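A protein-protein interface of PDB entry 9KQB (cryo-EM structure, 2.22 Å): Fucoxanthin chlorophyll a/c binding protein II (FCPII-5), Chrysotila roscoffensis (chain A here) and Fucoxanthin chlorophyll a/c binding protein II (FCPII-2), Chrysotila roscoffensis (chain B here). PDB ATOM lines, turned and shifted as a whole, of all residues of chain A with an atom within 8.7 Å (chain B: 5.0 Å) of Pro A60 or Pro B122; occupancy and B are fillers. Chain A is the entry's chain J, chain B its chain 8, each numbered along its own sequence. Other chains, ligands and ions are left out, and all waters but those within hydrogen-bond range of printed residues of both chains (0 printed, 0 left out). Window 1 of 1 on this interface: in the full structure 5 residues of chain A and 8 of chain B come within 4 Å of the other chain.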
ATOM      1  N   TYR A  57     -14.965 -27.219 -14.288  1.00  0.00           N
ATOM      2  CA  TYR A  57     -15.555 -25.907 -14.493  1.00  0.00           C
ATOM      3  C   TYR A  57     -17.073 -25.991 -14.550  1.00  0.00           C
ATOM      4  O   TYR A  57     -17.635 -26.909 -15.153  1.00  0.00           O
ATOM      5  CB  TYR A  57     -15.017 -25.242 -15.771  1.00  0.00           C
ATOM      6  CG  TYR A  57     -15.590 -23.862 -15.980  1.00  0.00           C
ATOM      7  CD1 TYR A  57     -15.075 -22.773 -15.293  1.00  0.00           C
ATOM      8  CD2 TYR A  57     -16.639 -23.648 -16.867  1.00  0.00           C
ATOM      9  CE1 TYR A  57     -15.597 -21.519 -15.467  1.00  0.00           C
ATOM     10  CE2 TYR A  57     -17.165 -22.398 -17.048  1.00  0.00           C
ATOM     11  CZ  TYR A  57     -16.639 -21.340 -16.347  1.00  0.00           C
ATOM     12  OH  TYR A  57     -17.163 -20.094 -16.529  1.00  0.00           O
ATOM     13  N   ARG A  58     -17.725 -25.016 -13.921  1.00  0.00           N
ATOM     14  CA  ARG A  58     -19.173 -24.873 -13.946  1.00  0.00           C
ATOM     15  C   ARG A  58     -19.524 -23.416 -14.213  1.00  0.00           C
ATOM     16  O   ARG A  58     -18.714 -22.510 -13.999  1.00  0.00           O
ATOM     17  CB  ARG A  58     -19.813 -25.334 -12.629  1.00  0.00           C
ATOM     18  CG  ARG A  58     -19.636 -26.812 -12.329  1.00  0.00           C
ATOM     19  CD  ARG A  58     -20.443 -27.673 -13.281  1.00  0.00           C
ATOM     20  NE  ARG A  58     -20.368 -29.086 -12.933  1.00  0.00           N
ATOM     21  CZ  ARG A  58     -21.137 -29.676 -12.028  1.00  0.00           C
ATOM     22  NH1 ARG A  58     -22.059 -29.004 -11.360  1.00  0.00           N
ATOM     23  NH2 ARG A  58     -20.976 -30.974 -11.789  1.00  0.00           N
ATOM     24  N   PHE A  59     -20.746 -23.197 -14.694  1.00  0.00           N
ATOM     25  CA  PHE A  59     -21.213 -21.847 -14.964  1.00  0.00           C
ATOM     26  C   PHE A  59     -21.457 -21.100 -13.649  1.00  0.00           C
ATOM     27  O   PHE A  59     -21.779 -21.715 -12.631  1.00  0.00           O
ATOM     28  CB  PHE A  59     -22.478 -21.893 -15.819  1.00  0.00           C
ATOM     29  CG  PHE A  59     -22.206 -22.159 -17.275  1.00  0.00           C
ATOM     30  CD1 PHE A  59     -21.259 -21.415 -17.961  1.00  0.00           C
ATOM     31  CD2 PHE A  59     -22.882 -23.161 -17.952  1.00  0.00           C
ATOM     32  CE1 PHE A  59     -20.998 -21.657 -19.297  1.00  0.00           C
ATOM     33  CE2 PHE A  59     -22.626 -23.409 -19.291  1.00  0.00           C
ATOM     34  CZ  PHE A  59     -21.683 -22.655 -19.962  1.00  0.00           C
ATOM     35  N   PRO A  60     -21.292 -19.771 -13.639  1.00  0.00           N
ATOM     36  CA  PRO A  60     -21.291 -19.055 -12.351  1.00  0.00           C
ATOM     37  C   PRO A  60     -22.658 -18.893 -11.704  1.00  0.00           C
ATOM     38  O   PRO A  60     -22.742 -18.914 -10.470  1.00  0.00           O
ATOM     39  CB  PRO A  60     -20.689 -17.691 -12.715  1.00  0.00           C
ATOM     40  CG  PRO A  60     -21.026 -17.513 -14.150  1.00  0.00           C
ATOM     41  CD  PRO A  60     -20.917 -18.880 -14.754  1.00  0.00           C
ATOM     42  N   GLY A  61     -23.727 -18.734 -12.478  1.00  0.00           N
ATOM     43  CA  GLY A  61     -25.010 -18.400 -11.888  1.00  0.00           C
ATOM     44  C   GLY A  61     -25.897 -19.576 -11.537  1.00  0.00           C
ATOM     45  O   GLY A  61     -25.413 -20.641 -11.142  1.00  0.00           O
ATOM     46  N   ILE A  62     -27.207 -19.376 -11.653  1.00  0.00           N
ATOM     47  CA  ILE A  62     -28.196 -20.422 -11.433  1.00  0.00           C
ATOM     48  C   ILE A  62     -28.817 -20.765 -12.777  1.00  0.00           C
ATOM     49  O   ILE A  62     -28.722 -19.993 -13.737  1.00  0.00           O
ATOM     50  CB  ILE A  62     -29.279 -19.996 -10.417  1.00  0.00           C
ATOM     51  CG1 ILE A  62     -30.208 -18.944 -11.030  1.00  0.00           C
ATOM     52  CG2 ILE A  62     -28.637 -19.471  -9.140  1.00  0.00           C
ATOM     53  CD1 ILE A  62     -31.217 -18.364 -10.060  1.00  0.00           C
ATOM     54  N   ILE A  63     -29.428 -21.945 -12.861  1.00  0.00           N
ATOM     55  CA  ILE A  63     -30.107 -22.304 -14.100  1.00  0.00           C
ATOM     56  C   ILE A  63     -31.608 -22.057 -13.984  1.00  0.00           C
ATOM     57  O   ILE A  63     -32.256 -21.625 -14.944  1.00  0.00           O
ATOM     58  CB  ILE A  63     -29.771 -23.756 -14.507  1.00  0.00           C
ATOM     59  CG1 ILE A  63     -30.368 -24.075 -15.880  1.00  0.00           C
ATOM     60  CG2 ILE A  63     -30.201 -24.765 -13.448  1.00  0.00           C
ATOM     61  CD1 ILE A  63     -29.552 -25.031 -16.690  1.00  0.00           C
ATOM     62  N   VAL A  67     -32.104 -23.153  -8.218  1.00  0.00           N
ATOM     63  CA  VAL A  67     -31.274 -24.234  -8.748  1.00  0.00           C
ATOM     64  C   VAL A  67     -29.956 -23.666  -9.261  1.00  0.00           C
ATOM     65  O   VAL A  67     -29.858 -23.301 -10.442  1.00  0.00           O
ATOM     66  CB  VAL A  67     -32.007 -25.006  -9.859  1.00  0.00           C
ATOM     67  CG1 VAL A  67     -31.290 -26.309 -10.162  1.00  0.00           C
ATOM     68  CG2 VAL A  67     -33.450 -25.289  -9.459  1.00  0.00           C
ATOM     69  N   PRO A  68     -28.929 -23.560  -8.420  1.00  0.00           N
ATOM     70  CA  PRO A  68     -27.630 -23.078  -8.901  1.00  0.00           C
ATOM     71  C   PRO A  68     -26.931 -24.101  -9.781  1.00  0.00           C
ATOM     72  O   PRO A  68     -27.226 -25.298  -9.745  1.00  0.00           O
ATOM     73  CB  PRO A  68     -26.842 -22.825  -7.609  1.00  0.00           C
ATOM     74  CG  PRO A  68     -27.881 -22.711  -6.539  1.00  0.00           C
ATOM     75  CD  PRO A  68     -28.966 -23.654  -6.953  1.00  0.00           C
ATOM     76  N   PHE A  69     -25.989 -23.603 -10.587  1.00  0.00           N
ATOM     77  CA  PHE A  69     -25.213 -24.474 -11.465  1.00  0.00           C
ATOM     78  C   PHE A  69     -24.268 -25.375 -10.680  1.00  0.00           C
ATOM     79  O   PHE A  69     -23.905 -26.456 -11.157  1.00  0.00           O
ATOM     80  CB  PHE A  69     -24.407 -23.637 -12.460  1.00  0.00           C
ATOM     81  CG  PHE A  69     -25.132 -23.328 -13.740  1.00  0.00           C
ATOM     82  CD1 PHE A  69     -25.059 -24.194 -14.815  1.00  0.00           C
ATOM     83  CD2 PHE A  69     -25.857 -22.157 -13.880  1.00  0.00           C
ATOM     84  CE1 PHE A  69     -25.717 -23.913 -15.999  1.00  0.00           C
ATOM     85  CE2 PHE A  69     -26.513 -21.869 -15.062  1.00  0.00           C
ATOM     86  CZ  PHE A  69     -26.444 -22.747 -16.121  1.00  0.00           C
ATOM     87  N   ALA A  70     -23.853 -24.943  -9.487  1.00  0.00           N
ATOM     88  CA  ALA A  70     -22.813 -25.657  -8.752  1.00  0.00           C
ATOM     89  C   ALA A  70     -23.322 -26.974  -8.178  1.00  0.00           C
ATOM     90  O   ALA A  70     -22.644 -28.004  -8.271  1.00  0.00           O
ATOM     91  CB  ALA A  70     -22.257 -24.767  -7.641  1.00  0.00           C
ATOM     92  N   LEU B  99     -26.101  -5.689 -12.452  1.00  0.00           N
ATOM     93  CA  LEU B  99     -25.586  -6.424 -13.600  1.00  0.00           C
ATOM     94  C   LEU B  99     -26.093  -7.859 -13.588  1.00  0.00           C
ATOM     95  O   LEU B  99     -26.353  -8.443 -14.647  1.00  0.00           O
ATOM     96  CB  LEU B  99     -24.056  -6.392 -13.601  1.00  0.00           C
ATOM     97  CG  LEU B  99     -23.319  -7.153 -14.705  1.00  0.00           C
ATOM     98  CD1 LEU B  99     -23.508  -6.473 -16.048  1.00  0.00           C
ATOM     99  CD2 LEU B  99     -21.841  -7.291 -14.374  1.00  0.00           C
ATOM    100  N   SER B 100     -26.255  -8.432 -12.396  1.00  0.00           N
ATOM    101  CA  SER B 100     -26.748  -9.798 -12.226  1.00  0.00           C
ATOM    102  C   SER B 100     -27.554  -9.838 -10.933  1.00  0.00           C
ATOM    103  O   SER B 100     -26.981  -9.811  -9.840  1.00  0.00           O
ATOM    104  CB  SER B 100     -25.602 -10.802 -12.193  1.00  0.00           C
ATOM    105  OG  SER B 100     -25.317 -11.294 -13.487  1.00  0.00           O
ATOM    106  N   LEU B 103     -26.815 -13.216  -9.107  1.00  0.00           N
ATOM    107  CA  LEU B 103     -25.540 -13.272  -8.411  1.00  0.00           C
ATOM    108  C   LEU B 103     -25.348 -12.109  -7.446  1.00  0.00           C
ATOM    109  O   LEU B 103     -24.280 -12.004  -6.830  1.00  0.00           O
ATOM    110  CB  LEU B 103     -24.392 -13.314  -9.421  1.00  0.00           C
ATOM    111  CG  LEU B 103     -24.223 -14.621 -10.193  1.00  0.00           C
ATOM    112  CD1 LEU B 103     -23.566 -14.370 -11.539  1.00  0.00           C
ATOM    113  CD2 LEU B 103     -23.419 -15.621  -9.381  1.00  0.00           C
ATOM    114  N   LEU B 105     -25.041  -8.910  -8.158  1.00  0.00           N
ATOM    115  CA  LEU B 105     -23.925  -8.165  -8.732  1.00  0.00           C
ATOM    116  C   LEU B 105     -24.436  -6.816  -9.222  1.00  0.00           C
ATOM    117  O   LEU B 105     -24.951  -6.704 -10.337  1.00  0.00           O
ATOM    118  CB  LEU B 105     -23.272  -8.952  -9.863  1.00  0.00           C
ATOM    119  CG  LEU B 105     -21.869  -8.492 -10.259  1.00  0.00           C
ATOM    120  CD1 LEU B 105     -20.970  -8.397  -9.038  1.00  0.00           C
ATOM    121  CD2 LEU B 105     -21.272  -9.432 -11.286  1.00  0.00           C
ATOM    122  N   THR B 120     -14.744 -10.015 -12.678  1.00  0.00           N
ATOM    123  CA  THR B 120     -15.963  -9.898 -11.882  1.00  0.00           C
ATOM    124  C   THR B 120     -17.216 -10.083 -12.730  1.00  0.00           C
ATOM    125  O   THR B 120     -18.245 -10.551 -12.227  1.00  0.00           O
ATOM    126  CB  THR B 120     -15.986  -8.549 -11.166  1.00  0.00           C
ATOM    127  OG1 THR B 120     -14.676  -8.264 -10.663  1.00  0.00           O
ATOM    128  CG2 THR B 120     -16.964  -8.568 -10.003  1.00  0.00           C
ATOM    129  N   VAL B 121     -17.158  -9.716 -14.007  1.00  0.00           N
ATOM    130  CA  VAL B 121     -18.317  -9.941 -14.880  1.00  0.00           C
ATOM    131  C   VAL B 121     -18.499 -11.440 -15.083  1.00  0.00           C
ATOM    132  O   VAL B 121     -17.520 -12.140 -15.408  1.00  0.00           O
ATOM    133  CB  VAL B 121     -18.134  -9.213 -16.223  1.00  0.00           C
ATOM    134  CG1 VAL B 121     -19.097  -9.752 -17.272  1.00  0.00           C
ATOM    135  CG2 VAL B 121     -18.363  -7.729 -16.035  1.00  0.00           C
ATOM    136  N   PRO B 122     -19.700 -11.984 -14.867  1.00  0.00           N
ATOM    137  CA  PRO B 122     -19.888 -13.434 -14.978  1.00  0.00           C
ATOM    138  C   PRO B 122     -19.668 -13.929 -16.398  1.00  0.00           C
ATOM    139  O   PRO B 122     -19.875 -13.207 -17.375  1.00  0.00           O
ATOM    140  CB  PRO B 122     -21.341 -13.641 -14.534  1.00  0.00           C
ATOM    141  CG  PRO B 122     -21.993 -12.320 -14.736  1.00  0.00           C
ATOM    142  CD  PRO B 122     -20.937 -11.298 -14.459  1.00  0.00           C
ATOM    143  N   VAL B 123     -19.215 -15.179 -16.488  1.00  0.00           N
ATOM    144  CA  VAL B 123     -18.885 -15.786 -17.770  1.00  0.00           C
ATOM    145  C   VAL B 123     -20.129 -15.976 -18.628  1.00  0.00           C
ATOM    146  O   VAL B 123     -20.055 -15.903 -19.861  1.00  0.00           O
ATOM    147  CB  VAL B 123     -18.128 -17.099 -17.513  1.00  0.00           C
ATOM    148  CG1 VAL B 123     -17.515 -17.630 -18.794  1.00  0.00           C
ATOM    149  CG2 VAL B 123     -17.045 -16.842 -16.475  1.00  0.00           C
ATOM    150  N   THR B 124     -21.286 -16.214 -18.004  1.00  0.00           N
ATOM    151  CA  THR B 124     -22.539 -16.223 -18.752  1.00  0.00           C
ATOM    152  C   THR B 124     -22.835 -14.843 -19.326  1.00  0.00           C
ATOM    153  O   THR B 124     -23.362 -14.723 -20.438  1.00  0.00           O
ATOM    154  CB  THR B 124     -23.684 -16.691 -17.858  1.00  0.00           C
ATOM    155  OG1 THR B 124     -23.625 -16.000 -16.604  1.00  0.00           O
ATOM    156  CG2 THR B 124     -23.587 -18.186 -17.609  1.00  0.00           C
ATOM    157  N   GLY B 125     -22.514 -13.790 -18.572  1.00  0.00           N
ATOM    158  CA  GLY B 125     -22.607 -12.445 -19.109  1.00  0.00           C
ATOM    159  C   GLY B 125     -21.595 -12.175 -20.203  1.00  0.00           C
ATOM    160  O   GLY B 125     -21.905 -11.487 -21.178  1.00  0.00           O
ATOM    161  N   TRP B 126     -20.378 -12.712 -20.062  1.00  0.00           N
ATOM    162  CA  TRP B 126     -19.354 -12.535 -21.089  1.00  0.00           C
ATOM    163  C   TRP B 126     -19.715 -13.280 -22.366  1.00  0.00           C
ATOM    164  O   TRP B 126     -19.345 -12.851 -23.466  1.00  0.00           O
ATOM    165  CB  TRP B 126     -17.995 -13.013 -20.577  1.00  0.00           C
ATOM    166  CG  TRP B 126     -17.171 -11.952 -19.916  1.00  0.00           C
ATOM    167  CD1 TRP B 126     -16.724 -11.953 -18.628  1.00  0.00           C
ATOM    168  CD2 TRP B 126     -16.676 -10.745 -20.510  1.00  0.00           C
ATOM    169  NE1 TRP B 126     -15.994 -10.819 -18.379  1.00  0.00           N
ATOM    170  CE2 TRP B 126     -15.949 -10.060 -19.519  1.00  0.00           C
ATOM    171  CE3 TRP B 126     -16.780 -10.175 -21.784  1.00  0.00           C
ATOM    172  CZ2 TRP B 126     -15.331  -8.835 -19.759  1.00  0.00           C
ATOM    173  CZ3 TRP B 126     -16.169  -8.959 -22.018  1.00  0.00           C
ATOM    174  CH2 TRP B 126     -15.453  -8.303 -21.011  1.00  0.00           C
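Of the 11 printed residues of chain A, 3 touch a printed residue of chain B. Among the printed residues, 6 pairs touch across the chains. Among the printed residues, no Asp or Glu carboxylate lies within 4 Å of a Lys or Arg side-chain nitrogen of the other chain.
Among the printed residues, pairs that only touch across the chains: Tyr A57 with Val B123 (3.3 Å), Pro A60 with Leu B103 (3.5 Å), Pro A60 with Val B123 (3.8 Å), Pro A60 with Thr B124 (3.9 Å), Pro A60 with Pro B122 (3.9 Å) and Phe A59 with Thr B124 (3.996 Å).
Of the printed residues of chain B, Tyr A57 touches Val B123 (3.3 Å). Of chain B, only Leu B103, Pro B122, Val B123 and Thr B124 come within 4 Å of Pro A60. Printed residues of chain A within 4 Å of Leu B103: Pro A60 (3.5 Å). No residue of chain A comes within 4 Å of Val B121. Of chain A, only Pro A60 (3.9 Å) comes within 4 Å of Pro B122. The nearest residue of chain A that does not touch Pro B122 is Gly A61 (6.0 Å). The nearest printed residue of chain B that does not touch Phe A59 is Val B123 (5.3 Å).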
